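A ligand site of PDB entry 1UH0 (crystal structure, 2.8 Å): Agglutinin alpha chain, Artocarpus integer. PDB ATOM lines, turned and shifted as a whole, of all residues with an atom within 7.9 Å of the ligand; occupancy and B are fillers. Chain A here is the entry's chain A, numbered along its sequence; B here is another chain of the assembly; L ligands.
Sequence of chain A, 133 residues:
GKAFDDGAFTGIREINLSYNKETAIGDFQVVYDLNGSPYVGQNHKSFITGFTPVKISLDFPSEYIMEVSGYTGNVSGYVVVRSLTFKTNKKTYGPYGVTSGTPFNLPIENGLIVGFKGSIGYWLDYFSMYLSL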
ATOM      1  N   GLY A   1      28.171 -21.922 -11.243  1.00  0.00           N
ATOM      2  CA  GLY A   1      28.974 -22.036 -10.007  1.00  0.00           C
ATOM      3  C   GLY A   1      29.254 -23.485  -9.675  1.00  0.00           C
ATOM      4  O   GLY A   1      28.747 -24.377 -10.346  1.00  0.00           O
ATOM      5  N   LYS A   2      30.053 -23.718  -8.640  1.00  0.00           N
ATOM      6  CA  LYS A   2      30.393 -25.073  -8.246  1.00  0.00           C
ATOM      7  C   LYS A   2      29.414 -25.548  -7.167  1.00  0.00           C
ATOM      8  O   LYS A   2      29.319 -24.946  -6.088  1.00  0.00           O
ATOM      9  CB  LYS A   2      31.835 -25.110  -7.732  1.00  0.00           C
ATOM     10  CG  LYS A   2      32.234 -26.508  -7.490  1.00  0.00           C
ATOM     11  CD  LYS A   2      33.502 -26.696  -6.787  1.00  0.00           C
ATOM     12  CE  LYS A   2      33.594 -28.177  -6.752  1.00  0.00           C
ATOM     13  NZ  LYS A   2      34.828 -28.281  -6.164  1.00  0.00           N
ATOM     14  N   ALA A  24      26.836  -9.592  -3.113  1.00  0.00           N
ATOM     15  CA  ALA A  24      26.051 -10.654  -2.504  1.00  0.00           C
ATOM     16  C   ALA A  24      26.874 -11.518  -1.540  1.00  0.00           C
ATOM     17  O   ALA A  24      27.975 -11.145  -1.153  1.00  0.00           O
ATOM     18  CB  ALA A  24      25.425 -11.530  -3.572  1.00  0.00           C
ATOM     19  N   ILE A  25      26.325 -12.673  -1.153  1.00  0.00           N
ATOM     20  CA  ILE A  25      27.014 -13.588  -0.243  1.00  0.00           C
ATOM     21  C   ILE A  25      28.140 -14.283  -1.001  1.00  0.00           C
ATOM     22  O   ILE A  25      27.970 -14.687  -2.151  1.00  0.00           O
ATOM     23  CB  ILE A  25      26.049 -14.644   0.314  1.00  0.00           C
ATOM     24  CG1 ILE A  25      24.894 -13.961   1.069  1.00  0.00           C
ATOM     25  CG2 ILE A  25      26.780 -15.591   1.248  1.00  0.00           C
ATOM     26  CD1 ILE A  25      25.324 -13.210   2.291  1.00  0.00           C
ATOM     27  N   SER A  46      34.100 -18.727  -2.870  1.00  0.00           N
ATOM     28  CA  SER A  46      33.796 -17.977  -4.079  1.00  0.00           C
ATOM     29  C   SER A  46      34.975 -18.018  -5.025  1.00  0.00           C
ATOM     30  O   SER A  46      36.124 -18.113  -4.601  1.00  0.00           O
ATOM     31  CB  SER A  46      33.494 -16.516  -3.741  1.00  0.00           C
ATOM     32  OG  SER A  46      33.554 -15.704  -4.900  1.00  0.00           O
ATOM     33  N   PHE A  47      34.700 -17.945  -6.325  1.00  0.00           N
ATOM     34  CA  PHE A  47      35.757 -17.955  -7.318  1.00  0.00           C
ATOM     35  C   PHE A  47      36.581 -16.691  -7.164  1.00  0.00           C
ATOM     36  O   PHE A  47      37.715 -16.633  -7.607  1.00  0.00           O
ATOM     37  CB  PHE A  47      35.173 -17.988  -8.728  1.00  0.00           C
ATOM     38  CG  PHE A  47      34.435 -19.257  -9.056  1.00  0.00           C
ATOM     39  CD1 PHE A  47      34.606 -20.403  -8.288  1.00  0.00           C
ATOM     40  CD2 PHE A  47      33.604 -19.328 -10.171  1.00  0.00           C
ATOM     41  CE1 PHE A  47      33.962 -21.590  -8.618  1.00  0.00           C
ATOM     42  CE2 PHE A  47      32.959 -20.501 -10.517  1.00  0.00           C
ATOM     43  CZ  PHE A  47      33.139 -21.639  -9.737  1.00  0.00           C
ATOM     44  N   ILE A  48      36.004 -15.672  -6.530  1.00  0.00           N
ATOM     45  CA  ILE A  48      36.727 -14.419  -6.319  1.00  0.00           C
ATOM     46  C   ILE A  48      36.923 -14.100  -4.828  1.00  0.00           C
ATOM     47  O   ILE A  48      36.475 -14.851  -3.959  1.00  0.00           O
ATOM     48  CB  ILE A  48      35.988 -13.233  -6.993  1.00  0.00           C
ATOM     49  CG1 ILE A  48      34.607 -13.058  -6.357  1.00  0.00           C
ATOM     50  CG2 ILE A  48      35.856 -13.482  -8.497  1.00  0.00           C
ATOM     51  CD1 ILE A  48      33.783 -11.951  -6.989  1.00  0.00           C
ATOM     52  N   VAL A  75      22.810  -9.824  -9.948  1.00  0.00           N
ATOM     53  CA  VAL A  75      24.133  -9.240  -9.818  1.00  0.00           C
ATOM     54  C   VAL A  75      24.898  -9.628 -11.075  1.00  0.00           C
ATOM     55  O   VAL A  75      25.154 -10.806 -11.318  1.00  0.00           O
ATOM     56  CB  VAL A  75      24.868  -9.753  -8.571  1.00  0.00           C
ATOM     57  CG1 VAL A  75      26.261  -9.144  -8.526  1.00  0.00           C
ATOM     58  CG2 VAL A  75      24.073  -9.375  -7.327  1.00  0.00           C
ATOM     59  N   SER A  76      25.253  -8.623 -11.878  1.00  0.00           N
ATOM     60  CA  SER A  76      25.954  -8.842 -13.138  1.00  0.00           C
ATOM     61  C   SER A  76      25.218  -9.788 -14.029  1.00  0.00           C
ATOM     62  O   SER A  76      25.849 -10.583 -14.724  1.00  0.00           O
ATOM     63  CB  SER A  76      27.298  -9.505 -12.942  1.00  0.00           C
ATOM     64  OG  SER A  76      28.365  -8.564 -12.950  1.00  0.00           O
ATOM     65  N   GLY A  77      23.898  -9.758 -13.958  1.00  0.00           N
ATOM     66  CA  GLY A  77      23.126 -10.647 -14.796  1.00  0.00           C
ATOM     67  C   GLY A  77      22.850 -12.029 -14.211  1.00  0.00           C
ATOM     68  O   GLY A  77      22.142 -12.819 -14.820  1.00  0.00           O
ATOM     69  N   TYR A  78      23.378 -12.327 -13.040  1.00  0.00           N
ATOM     70  CA  TYR A  78      23.135 -13.627 -12.436  1.00  0.00           C
ATOM     71  C   TYR A  78      22.193 -13.492 -11.270  1.00  0.00           C
ATOM     72  O   TYR A  78      22.269 -12.523 -10.516  1.00  0.00           O
ATOM     73  CB  TYR A  78      24.435 -14.241 -11.932  1.00  0.00           C
ATOM     74  CG  TYR A  78      25.482 -14.463 -12.994  1.00  0.00           C
ATOM     75  CD1 TYR A  78      25.451 -15.588 -13.813  1.00  0.00           C
ATOM     76  CD2 TYR A  78      26.515 -13.536 -13.179  1.00  0.00           C
ATOM     77  CE1 TYR A  78      26.413 -15.796 -14.790  1.00  0.00           C
ATOM     78  CE2 TYR A  78      27.497 -13.732 -14.154  1.00  0.00           C
ATOM     79  CZ  TYR A  78      27.436 -14.864 -14.955  1.00  0.00           C
ATOM     80  OH  TYR A  78      28.399 -15.085 -15.915  1.00  0.00           O
ATOM     81  N   VAL A  79      21.293 -14.455 -11.100  1.00  0.00           N
ATOM     82  CA  VAL A  79      20.401 -14.432  -9.959  1.00  0.00           C
ATOM     83  C   VAL A  79      21.136 -15.146  -8.829  1.00  0.00           C
ATOM     84  O   VAL A  79      21.567 -16.287  -8.979  1.00  0.00           O
ATOM     85  CB  VAL A  79      19.086 -15.165 -10.246  1.00  0.00           C
ATOM     86  CG1 VAL A  79      18.307 -15.361  -8.957  1.00  0.00           C
ATOM     87  CG2 VAL A  79      18.269 -14.378 -11.237  1.00  0.00           C
ATOM     88  N   VAL A  80      21.295 -14.470  -7.699  1.00  0.00           N
ATOM     89  CA  VAL A  80      22.017 -15.031  -6.565  1.00  0.00           C
ATOM     90  C   VAL A  80      21.402 -14.670  -5.220  1.00  0.00           C
ATOM     91  O   VAL A  80      20.424 -13.918  -5.156  1.00  0.00           O
ATOM     92  CB  VAL A  80      23.482 -14.541  -6.557  1.00  0.00           C
ATOM     93  CG1 VAL A  80      24.190 -14.935  -7.857  1.00  0.00           C
ATOM     94  CG2 VAL A  80      23.522 -13.034  -6.379  1.00  0.00           C
ATOM     95  N   VAL A  81      21.985 -15.217  -4.157  1.00  0.00           N
ATOM     96  CA  VAL A  81      21.506 -14.936  -2.808  1.00  0.00           C
ATOM     97  C   VAL A  81      22.294 -13.726  -2.338  1.00  0.00           C
ATOM     98  O   VAL A  81      23.467 -13.841  -2.000  1.00  0.00           O
ATOM     99  CB  VAL A  81      21.785 -16.125  -1.853  1.00  0.00           C
ATOM    100  CG1 VAL A  81      21.224 -15.836  -0.483  1.00  0.00           C
ATOM    101  CG2 VAL A  81      21.144 -17.386  -2.404  1.00  0.00           C
ATOM    102  N   SER A 119      25.121 -23.913  -4.363  1.00  0.00           N
ATOM    103  CA  SER A 119      26.101 -23.692  -5.407  1.00  0.00           C
ATOM    104  C   SER A 119      26.755 -22.336  -5.224  1.00  0.00           C
ATOM    105  O   SER A 119      26.120 -21.380  -4.790  1.00  0.00           O
ATOM    106  CB  SER A 119      25.406 -23.745  -6.772  1.00  0.00           C
ATOM    107  OG  SER A 119      26.295 -23.400  -7.810  1.00  0.00           O
ATOM    108  N   ILE A 120      28.044 -22.262  -5.538  1.00  0.00           N
ATOM    109  CA  ILE A 120      28.770 -21.010  -5.419  1.00  0.00           C
ATOM    110  C   ILE A 120      29.712 -20.771  -6.603  1.00  0.00           C
ATOM    111  O   ILE A 120      30.554 -21.605  -6.904  1.00  0.00           O
ATOM    112  CB  ILE A 120      29.608 -20.973  -4.107  1.00  0.00           C
ATOM    113  CG1 ILE A 120      28.699 -21.132  -2.894  1.00  0.00           C
ATOM    114  CG2 ILE A 120      30.339 -19.654  -4.003  1.00  0.00           C
ATOM    115  CD1 ILE A 120      29.441 -21.157  -1.577  1.00  0.00           C
ATOM    116  N   GLY A 121      29.539 -19.628  -7.269  1.00  0.00           N
ATOM    117  CA  GLY A 121      30.408 -19.255  -8.393  1.00  0.00           C
ATOM    118  C   GLY A 121      31.153 -18.028  -7.879  1.00  0.00           C
ATOM    119  O   GLY A 121      32.021 -18.174  -7.019  1.00  0.00           O
ATOM    120  N   TYR A 122      30.829 -16.837  -8.362  1.00  0.00           N
ATOM    121  CA  TYR A 122      31.455 -15.629  -7.854  1.00  0.00           C
ATOM    122  C   TYR A 122      30.669 -15.365  -6.554  1.00  0.00           C
ATOM    123  O   TYR A 122      31.182 -14.782  -5.605  1.00  0.00           O
ATOM    124  CB  TYR A 122      31.276 -14.513  -8.906  1.00  0.00           C
ATOM    125  CG  TYR A 122      32.344 -14.258  -9.972  1.00  0.00           C
ATOM    126  CD1 TYR A 122      33.066 -15.242 -10.524  1.00  0.00           C
ATOM    127  CD2 TYR A 122      32.519 -13.015 -10.488  1.00  0.00           C
ATOM    128  CE1 TYR A 122      33.942 -14.988 -11.572  1.00  0.00           C
ATOM    129  CE2 TYR A 122      33.386 -12.774 -11.529  1.00  0.00           C
ATOM    130  CZ  TYR A 122      34.088 -13.762 -12.071  1.00  0.00           C
ATOM    131  OH  TYR A 122      34.966 -13.544 -13.097  1.00  0.00           O
ATOM    132  N   TRP A 123      29.419 -15.803  -6.527  1.00  0.00           N
ATOM    133  CA  TRP A 123      28.544 -15.640  -5.364  1.00  0.00           C
ATOM    134  C   TRP A 123      27.706 -16.900  -5.086  1.00  0.00           C
ATOM    135  O   TRP A 123      27.740 -17.853  -5.866  1.00  0.00           O
ATOM    136  CB  TRP A 123      27.589 -14.447  -5.557  1.00  0.00           C
ATOM    137  CG  TRP A 123      28.317 -13.195  -5.848  1.00  0.00           C
ATOM    138  CD1 TRP A 123      29.029 -12.431  -4.978  1.00  0.00           C
ATOM    139  CD2 TRP A 123      28.460 -12.593  -7.135  1.00  0.00           C
ATOM    140  NE1 TRP A 123      29.616 -11.374  -5.643  1.00  0.00           N
ATOM    141  CE2 TRP A 123      29.283 -11.448  -6.957  1.00  0.00           C
ATOM    142  CE3 TRP A 123      27.993 -12.881  -8.417  1.00  0.00           C
ATOM    143  CZ2 TRP A 123      29.630 -10.608  -8.033  1.00  0.00           C
ATOM    144  CZ3 TRP A 123      28.340 -12.046  -9.474  1.00  0.00           C
ATOM    145  CH2 TRP A 123      29.154 -10.925  -9.281  1.00  0.00           C
ATOM    146  N   LEU A 124      26.956 -16.888  -3.976  1.00  0.00           N
ATOM    147  CA  LEU A 124      26.075 -18.011  -3.638  1.00  0.00           C
ATOM    148  C   LEU A 124      24.891 -18.000  -4.615  1.00  0.00           C
ATOM    149  O   LEU A 124      23.995 -17.168  -4.511  1.00  0.00           O
ATOM    150  CB  LEU A 124      25.585 -17.878  -2.189  1.00  0.00           C
ATOM    151  CG  LEU A 124      24.597 -18.901  -1.604  1.00  0.00           C
ATOM    152  CD1 LEU A 124      25.205 -20.305  -1.616  1.00  0.00           C
ATOM    153  CD2 LEU A 124      24.236 -18.505  -0.175  1.00  0.00           C
ATOM    154  N   ASP A 125      24.907 -18.915  -5.571  1.00  0.00           N
ATOM    155  CA  ASP A 125      23.841 -18.993  -6.567  1.00  0.00           C
ATOM    156  C   ASP A 125      22.497 -19.361  -5.972  1.00  0.00           C
ATOM    157  O   ASP A 125      21.488 -18.715  -6.229  1.00  0.00           O
ATOM    158  CB  ASP A 125      24.221 -20.003  -7.642  1.00  0.00           C
ATOM    159  CG  ASP A 125      25.552 -19.709  -8.275  1.00  0.00           C
ATOM    160  OD1 ASP A 125      25.692 -18.619  -8.857  1.00  0.00           O
ATOM    161  OD2 ASP A 125      26.471 -20.546  -8.165  1.00  0.00           O
ATOM    162  N   TYR A 126      22.499 -20.428  -5.167  1.00  0.00           N
ATOM    163  CA  TYR A 126      21.282 -20.891  -4.510  1.00  0.00           C
ATOM    164  C   TYR A 126      21.655 -21.839  -3.397  1.00  0.00           C
ATOM    165  O   TYR A 126      22.811 -22.265  -3.282  1.00  0.00           O
ATOM    166  CB  TYR A 126      20.401 -21.616  -5.527  1.00  0.00           C
ATOM    167  CG  TYR A 126      21.053 -22.831  -6.132  1.00  0.00           C
ATOM    168  CD1 TYR A 126      21.207 -24.010  -5.402  1.00  0.00           C
ATOM    169  CD2 TYR A 126      21.554 -22.790  -7.438  1.00  0.00           C
ATOM    170  CE1 TYR A 126      21.829 -25.117  -5.952  1.00  0.00           C
ATOM    171  CE2 TYR A 126      22.196 -23.902  -8.000  1.00  0.00           C
ATOM    172  CZ  TYR A 126      22.328 -25.056  -7.254  1.00  0.00           C
ATOM    173  OH  TYR A 126      22.949 -26.162  -7.804  1.00  0.00           O
ATOM    174  N   ALA B  17      19.192 -18.584  -7.594  1.00  0.00           N
ATOM    175  CA  ALA B  17      19.136 -18.929  -9.006  1.00  0.00           C
ATOM    176  C   ALA B  17      18.367 -20.226  -9.218  1.00  0.00           C
ATOM    177  O   ALA B  17      18.522 -21.176  -8.457  1.00  0.00           O
ATOM    178  CB  ALA B  17      20.542 -19.080  -9.554  1.00  0.00           C
HETATM  179  O1  LIG L   1      27.505 -16.607  -8.612  1.00  0.00           O
HETATM  180  C1  LIG L   1      27.448 -16.350 -10.000  1.00  0.00           C
HETATM  181  C2  LIG L   1      27.963 -16.955 -11.310  1.00  0.00           C
HETATM  182  O2  LIG L   1      29.411 -16.990 -11.308  1.00  0.00           O
HETATM  183  C3  LIG L   1      30.064 -17.510 -12.483  1.00  0.00           C
HETATM  184  O3  LIG L   1      30.112 -16.490 -13.472  1.00  0.00           O
HETATM  185  C4  LIG L   1      30.806 -15.285 -13.794  1.00  0.00           C
HETATM  186  C5  LIG L   1      29.509 -18.940 -12.754  1.00  0.00           C
HETATM  187  N1  LIG L   1      29.964 -19.437 -14.060  1.00  0.00           N
HETATM  188  C6  LIG L   1      30.766 -20.546 -13.982  1.00  0.00           C
HETATM  189  O4  LIG L   1      31.088 -21.095 -12.923  1.00  0.00           O
HETATM  190  C7  LIG L   1      31.269 -21.130 -15.298  1.00  0.00           C
HETATM  191  C8  LIG L   1      27.975 -18.943 -12.806  1.00  0.00           C
HETATM  192  O5  LIG L   1      27.499 -20.258 -13.049  1.00  0.00           O
HETATM  193  C9  LIG L   1      27.425 -18.394 -11.489  1.00  0.00           C
HETATM  194  O6  LIG L   1      27.781 -19.244 -10.405  1.00  0.00           O
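The backbone NH (N) of Gly 1 sits at hydrogen-bond distance from an oxygen (O5) of the ligand, 2.5 Å away. The side-chain carboxylate (OD1) of Asp 125 sits at hydrogen-bond distance from an oxygen (O6) of the ligand. N of Trp 123 sits at hydrogen-bond distance from O1 of the ligand (2.9 Å). An oxygen (O1) of the ligand is in hydrogen-bond range of the backbone carbonyl oxygen (O) of Trp 123. O3 of the ligand sits close to OH of Tyr 78 (3.3 Å). N of Tyr 122 lies within hydrogen-bond range of O2 of the ligand (3.3 Å).
OD2 of Asp 125 is in hydrogen-bond range of N of Gly 121, 3.3 Å away. N of Phe 47 is in hydrogen-bond range of O of Gly 121 (2.8 Å). O of Tyr 122 is in hydrogen-bond range of OG of Ser 46 (2.6 Å). The backbone NH (N) of Asp 125 sits at hydrogen-bond distance from the backbone carbonyl oxygen (O) of Ser 119, 2.9 Å away. N of Ala 17 of chain B is in hydrogen-bond range of O of Asp 125 (2.7 Å).
Residues that only touch the ligand: Phe 47, Gly 121 and Val 80. Hydrophobic or aromatic side chains within 4 Å of the ligand: Phe 47, Tyr 78, Val 80, Tyr 122 and Trp 123. Within 4 Å of the ligand: Gly 1, Phe 47, Tyr 78, Val 80, Gly 121, Tyr 122, Trp 123 and Asp 125.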
